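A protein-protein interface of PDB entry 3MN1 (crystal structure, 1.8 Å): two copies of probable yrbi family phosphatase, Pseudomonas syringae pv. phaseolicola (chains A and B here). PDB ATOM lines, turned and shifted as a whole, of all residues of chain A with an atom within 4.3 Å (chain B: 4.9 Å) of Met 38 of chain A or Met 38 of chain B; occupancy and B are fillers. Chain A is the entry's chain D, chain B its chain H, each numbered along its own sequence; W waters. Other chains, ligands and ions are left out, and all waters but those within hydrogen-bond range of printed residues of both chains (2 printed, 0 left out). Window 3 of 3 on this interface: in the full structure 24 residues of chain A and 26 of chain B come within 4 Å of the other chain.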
ATOM      1  N   PHE A  37     -17.573   5.244 -15.625  1.00  0.00           N
ATOM      2  CA  PHE A  37     -17.205   5.015 -17.022  1.00  0.00           C
ATOM      3  C   PHE A  37     -16.282   6.084 -17.544  1.00  0.00           C
ATOM      4  O   PHE A  37     -16.476   7.274 -17.284  1.00  0.00           O
ATOM      5  CB  PHE A  37     -18.447   4.947 -17.914  1.00  0.00           C
ATOM      6  CG  PHE A  37     -19.323   3.779 -17.632  1.00  0.00           C
ATOM      7  CD1 PHE A  37     -19.057   2.543 -18.203  1.00  0.00           C
ATOM      8  CD2 PHE A  37     -20.422   3.908 -16.802  1.00  0.00           C
ATOM      9  CE1 PHE A  37     -19.876   1.455 -17.954  1.00  0.00           C
ATOM     10  CE2 PHE A  37     -21.247   2.823 -16.544  1.00  0.00           C
ATOM     11  CZ  PHE A  37     -20.976   1.595 -17.122  1.00  0.00           C
ATOM     12  N   MET A  38     -15.259   5.661 -18.272  1.00  0.00           N
ATOM     13  CA  MET A  38     -14.365   6.610 -18.894  1.00  0.00           C
ATOM     14  C   MET A  38     -14.836   6.855 -20.337  1.00  0.00           C
ATOM     15  O   MET A  38     -15.721   6.146 -20.854  1.00  0.00           O
ATOM     16  CB  MET A  38     -12.921   6.101 -18.837  1.00  0.00           C
ATOM     17  CG  MET A  38     -12.546   5.500 -17.467  1.00  0.00           C
ATOM     18  SD  MET A  38     -10.810   5.012 -17.369  1.00  0.00           S
ATOM     19  CE  MET A  38     -10.081   6.610 -17.523  1.00  0.00           C
ATOM     20  N   GLU A  39     -14.266   7.869 -20.971  1.00  0.00           N
ATOM     21  CA  GLU A  39     -14.639   8.223 -22.337  1.00  0.00           C
ATOM     22  C   GLU A  39     -14.430   7.075 -23.309  1.00  0.00           C
ATOM     23  O   GLU A  39     -15.262   6.844 -24.187  1.00  0.00           O
ATOM     24  CB  GLU A  39     -13.841   9.430 -22.816  1.00  0.00           C
ATOM     25  CG  GLU A  39     -14.461  10.742 -22.462  1.00  0.00           C
ATOM     26  CD  GLU A  39     -13.572  11.894 -22.854  1.00  0.00           C
ATOM     27  OE1 GLU A  39     -12.625  11.676 -23.647  1.00  0.00           O
ATOM     28  OE2 GLU A  39     -13.813  13.009 -22.362  1.00  0.00           O
ATOM     29  N   ASP A  40     -13.311   6.370 -23.160  1.00  0.00           N
ATOM     30  CA  ASP A  40     -13.003   5.243 -24.036  1.00  0.00           C
ATOM     31  C   ASP A  40     -13.855   4.006 -23.753  1.00  0.00           C
ATOM     32  O   ASP A  40     -13.653   2.959 -24.370  1.00  0.00           O
ATOM     33  CB  ASP A  40     -11.509   4.888 -23.983  1.00  0.00           C
ATOM     34  CG  ASP A  40     -11.086   4.296 -22.642  1.00  0.00           C
ATOM     35  OD1 ASP A  40     -11.952   4.119 -21.751  1.00  0.00           O
ATOM     36  OD2 ASP A  40      -9.878   4.007 -22.481  1.00  0.00           O
ATOM     37  N   GLY A  41     -14.803   4.121 -22.823  1.00  0.00           N
ATOM     38  CA  GLY A  41     -15.763   3.046 -22.571  1.00  0.00           C
ATOM     39  C   GLY A  41     -15.377   2.080 -21.455  1.00  0.00           C
ATOM     40  O   GLY A  41     -16.180   1.251 -21.028  1.00  0.00           O
ATOM     41  N   SER A  42     -14.147   2.177 -20.977  1.00  0.00           N
ATOM     42  CA  SER A  42     -13.700   1.270 -19.923  1.00  0.00           C
ATOM     43  C   SER A  42     -14.263   1.678 -18.543  1.00  0.00           C
ATOM     44  O   SER A  42     -14.722   2.813 -18.351  1.00  0.00           O
ATOM     45  CB  SER A  42     -12.180   1.205 -19.898  1.00  0.00           C
ATOM     46  OG  SER A  42     -11.651   2.466 -19.559  1.00  0.00           O
ATOM     47  N   GLU A  43     -14.247   0.741 -17.595  1.00  0.00           N
ATOM     48  CA  GLU A  43     -14.818   0.997 -16.283  1.00  0.00           C
ATOM     49  C   GLU A  43     -13.769   1.126 -15.188  1.00  0.00           C
ATOM     50  O   GLU A  43     -12.638   0.654 -15.323  1.00  0.00           O
ATOM     51  CB  GLU A  43     -15.802  -0.114 -15.922  1.00  0.00           C
ATOM     52  CG  GLU A  43     -16.950  -0.224 -16.902  1.00  0.00           C
ATOM     53  CD  GLU A  43     -17.815  -1.449 -16.664  1.00  0.00           C
ATOM     54  OE1 GLU A  43     -18.578  -1.458 -15.675  1.00  0.00           O
ATOM     55  OE2 GLU A  43     -17.739  -2.393 -17.482  1.00  0.00           O
ATOM     56  N   ILE A  44     -14.159   1.791 -14.102  1.00  0.00           N
ATOM     57  CA  ILE A  44     -13.405   1.790 -12.851  1.00  0.00           C
ATOM     58  C   ILE A  44     -14.371   1.244 -11.808  1.00  0.00           C
ATOM     59  O   ILE A  44     -15.581   1.494 -11.866  1.00  0.00           O
ATOM     60  CB  ILE A  44     -12.985   3.220 -12.458  1.00  0.00           C
ATOM     61  CG1 ILE A  44     -12.045   3.793 -13.522  1.00  0.00           C
ATOM     62  CG2 ILE A  44     -12.283   3.240 -11.104  1.00  0.00           C
ATOM     63  CD1 ILE A  44     -11.870   5.278 -13.415  1.00  0.00           C
ATOM     64  N   ILE A  75     -12.209  -6.729 -13.672  1.00  0.00           N
ATOM     65  CA  ILE A  75     -11.923  -6.092 -12.388  1.00  0.00           C
ATOM     66  C   ILE A  75     -12.466  -6.972 -11.266  1.00  0.00           C
ATOM     67  O   ILE A  75     -11.815  -7.159 -10.224  1.00  0.00           O
ATOM     68  CB  ILE A  75     -12.604  -4.709 -12.283  1.00  0.00           C
ATOM     69  CG1 ILE A  75     -12.000  -3.715 -13.283  1.00  0.00           C
ATOM     70  CG2 ILE A  75     -12.499  -4.155 -10.854  1.00  0.00           C
ATOM     71  CD1 ILE A  75     -12.785  -2.392 -13.380  1.00  0.00           C
ATOM     72  N   TYR B  36      -9.936   1.837  -5.643  1.00  0.00           N
ATOM     73  CA  TYR B  36     -10.343   2.024  -7.033  1.00  0.00           C
ATOM     74  C   TYR B  36      -9.449   1.183  -7.950  1.00  0.00           C
ATOM     75  O   TYR B  36      -8.222   1.257  -7.856  1.00  0.00           O
ATOM     76  CB  TYR B  36     -10.123   3.468  -7.450  1.00  0.00           C
ATOM     77  CG  TYR B  36     -10.958   4.515  -6.746  1.00  0.00           C
ATOM     78  CD1 TYR B  36     -11.996   5.147  -7.408  1.00  0.00           C
ATOM     79  CD2 TYR B  36     -10.670   4.915  -5.438  1.00  0.00           C
ATOM     80  CE1 TYR B  36     -12.747   6.126  -6.794  1.00  0.00           C
ATOM     81  CE2 TYR B  36     -11.418   5.905  -4.816  1.00  0.00           C
ATOM     82  CZ  TYR B  36     -12.457   6.505  -5.500  1.00  0.00           C
ATOM     83  OH  TYR B  36     -13.214   7.491  -4.887  1.00  0.00           O
ATOM     84  N   PHE B  37     -10.050   0.413  -8.848  1.00  0.00           N
ATOM     85  CA  PHE B  37      -9.270  -0.377  -9.797  1.00  0.00           C
ATOM     86  C   PHE B  37      -9.756  -0.132 -11.218  1.00  0.00           C
ATOM     87  O   PHE B  37     -10.964  -0.061 -11.477  1.00  0.00           O
ATOM     88  CB  PHE B  37      -9.387  -1.867  -9.498  1.00  0.00           C
ATOM     89  CG  PHE B  37      -8.806  -2.279  -8.182  1.00  0.00           C
ATOM     90  CD1 PHE B  37      -7.455  -2.577  -8.075  1.00  0.00           C
ATOM     91  CD2 PHE B  37      -9.623  -2.427  -7.061  1.00  0.00           C
ATOM     92  CE1 PHE B  37      -6.913  -2.995  -6.870  1.00  0.00           C
ATOM     93  CE2 PHE B  37      -9.090  -2.840  -5.848  1.00  0.00           C
ATOM     94  CZ  PHE B  37      -7.733  -3.131  -5.754  1.00  0.00           C
ATOM     95  N   MET B  38      -8.814   0.006 -12.143  1.00  0.00           N
ATOM     96  CA  MET B  38      -9.164   0.051 -13.548  1.00  0.00           C
ATOM     97  C   MET B  38      -9.105  -1.362 -14.130  1.00  0.00           C
ATOM     98  O   MET B  38      -8.656  -2.311 -13.470  1.00  0.00           O
ATOM     99  CB  MET B  38      -8.251   1.027 -14.294  1.00  0.00           C
ATOM    100  CG  MET B  38      -8.285   2.446 -13.694  1.00  0.00           C
ATOM    101  SD  MET B  38      -7.103   3.589 -14.431  1.00  0.00           S
ATOM    102  CE  MET B  38      -7.956   3.932 -15.952  1.00  0.00           C
ATOM    103  N   GLU B  39      -9.579  -1.513 -15.360  1.00  0.00           N
ATOM    104  CA  GLU B  39      -9.703  -2.844 -15.954  1.00  0.00           C
ATOM    105  C   GLU B  39      -8.404  -3.638 -16.014  1.00  0.00           C
ATOM    106  O   GLU B  39      -8.426  -4.856 -15.896  1.00  0.00           O
ATOM    107  CB  GLU B  39     -10.316  -2.748 -17.346  1.00  0.00           C
ATOM    108  CG  GLU B  39     -11.821  -2.705 -17.324  1.00  0.00           C
ATOM    109  CD  GLU B  39     -12.410  -2.165 -18.610  1.00  0.00           C
ATOM    110  OE1 GLU B  39     -11.734  -2.243 -19.665  1.00  0.00           O
ATOM    111  OE2 GLU B  39     -13.557  -1.671 -18.568  1.00  0.00           O
ATOM    112  N   ASP B  40      -7.276  -2.958 -16.188  1.00  0.00           N
ATOM    113  CA  ASP B  40      -5.989  -3.659 -16.235  1.00  0.00           C
ATOM    114  C   ASP B  40      -5.389  -3.890 -14.845  1.00  0.00           C
ATOM    115  O   ASP B  40      -4.258  -4.364 -14.710  1.00  0.00           O
ATOM    116  CB  ASP B  40      -4.990  -2.919 -17.127  1.00  0.00           C
ATOM    117  CG  ASP B  40      -4.563  -1.579 -16.555  1.00  0.00           C
ATOM    118  OD1 ASP B  40      -4.988  -1.226 -15.436  1.00  0.00           O
ATOM    119  OD2 ASP B  40      -3.796  -0.870 -17.238  1.00  0.00           O
ATOM    120  N   GLY B  41      -6.134  -3.540 -13.805  1.00  0.00           N
ATOM    121  CA  GLY B  41      -5.651  -3.770 -12.444  1.00  0.00           C
ATOM    122  C   GLY B  41      -4.924  -2.596 -11.807  1.00  0.00           C
ATOM    123  O   GLY B  41      -4.563  -2.658 -10.625  1.00  0.00           O
ATOM    124  N   SER B  42      -4.683  -1.539 -12.572  1.00  0.00           N
ATOM    125  CA  SER B  42      -4.019  -0.355 -12.012  1.00  0.00           C
ATOM    126  C   SER B  42      -4.968   0.350 -11.036  1.00  0.00           C
ATOM    127  O   SER B  42      -6.184   0.246 -11.172  1.00  0.00           O
ATOM    128  CB  SER B  42      -3.563   0.602 -13.116  1.00  0.00           C
ATOM    129  OG  SER B  42      -4.665   1.055 -13.853  1.00  0.00           O
ATOM    130  N   ILE B  44      -6.237   3.665  -8.333  1.00  0.00           N
ATOM    131  CA  ILE B  44      -6.358   5.094  -8.053  1.00  0.00           C
ATOM    132  C   ILE B  44      -6.549   5.161  -6.553  1.00  0.00           C
ATOM    133  O   ILE B  44      -7.170   4.274  -5.957  1.00  0.00           O
ATOM    134  CB  ILE B  44      -7.609   5.705  -8.713  1.00  0.00           C
ATOM    135  CG1 ILE B  44      -7.596   5.458 -10.217  1.00  0.00           C
ATOM    136  CG2 ILE B  44      -7.706   7.217  -8.385  1.00  0.00           C
ATOM    137  CD1 ILE B  44      -8.842   5.914 -10.922  1.00  0.00           C
HETATM  138  O   HOH W   1     -14.923  -3.557 -17.164  1.00  0.00           O
HETATM  139  O   HOH W   2     -10.533   0.548 -16.667  1.00  0.00           O
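Of the 8 printed residues of chain B, 4 touch a printed residue of chain A. Hydrophobic or aromatic side chains of chain A within 4 Å of the printed part of chain B: Met 38, Ile 44 and Ile 75. Among the printed residues, no Asp or Glu carboxylate lies within 4 Å of a Lys or Arg side-chain nitrogen of the other chain.
Met 38 of chain A touches its own counterpart, Met 38 of chain B. Ile 44 of chain A touches Phe 37 of chain B, but with the chains exchanged Phe 37 of chain A does not touch Ile 44 of chain B (9.9 Å). Ile 44 of chain A touches Met 38 of chain B, but with the chains exchanged Met 38 of chain A does not touch Ile 44 of chain B (6.8 Å). Ile 44 of chain B touches its own counterpart, Ile 44 of chain A. Of the 10 pairs that touch across the chains among the printed residues, 2 have their exchanged pair printed and touching as well.
Printed residues of chain B within 4 Å of Met 38 of chain A: Met 38. Of the printed residues of chain B, Ile 44 of chain A touches Phe 37 (3.4 Å), Met 38 (3.998 Å) and Ile 44 (3.97 Å). Of the printed residues of chain B, Ile 75 of chain A touches Phe 37, Met 38 and Glu 39. Of the printed residues of chain A, Met 38 of chain B touches Met 38, Glu 43, Ile 44 and Ile 75. Ser 42 of chain B touches none of the printed residues of chain A. The nearest printed residue of chain B that does not touch Met 38 of chain A is Ile 44 of chain B (6.8 Å). The nearest printed residue of chain A that does not touch Met 38 of chain B is Ser 42 of chain A (5.4 Å).
The side-chain hydroxyl of Ser 42 of chain B is in hydrogen-bond range of the side-chain sulfur of Met 38 of chain B (3.6 Å). O of Tyr 36 of chain B is in hydrogen-bond range of N of Ile 44 of chain B, at 3.2 Å. SD of Met 38 of chain A sits at hydrogen-bond distance from OG of Ser 42 of chain A, at 3.5 Å. OD1 of Asp 40 of chain A is in hydrogen-bond range of OG of Ser 42 of chain A (2.8 Å).
Water W2 lies within hydrogen-bond range of the backbone carbonyl oxygen of Glu 43 of chain A (2.5 Å) and the backbone NH of Glu 39 of chain B (2.6 Å). Water W1 bridges OE2 of Glu 39 of chain B (2.7 Å) and OE2 of Glu 43 of chain A (3.1 Å).
The backbone NH (N) of Glu 43 of chain A is in hydrogen-bond range of the side-chain carboxylate (OE2) of Glu 39 of chain B.
Met 38 of chain B touches Met 38 of chain A (CE to SD, 3.4 Å). CA of Ser 42 of chain A touches OE2 of Glu 39 of chain B (3.2 Å). Glu 43 of chain A touches Met 38 of chain B (O to CA, 3.9 Å). Ile 44 of chain A touches Phe 37 of chain B (CA to O, 3.4 Å). Met 38 of chain B touches Ile 44 of chain A. CD1 of Ile 44 of chain B touches CD1 of Ile 44 of chain A, at 3.97 Å. Phe 37 of chain B touches Ile 75 of chain A. CG1 of Ile 75 of chain A touches O of Met 38 of chain B (3.6 Å). Ile 75 of chain A touches Glu 39 of chain B.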
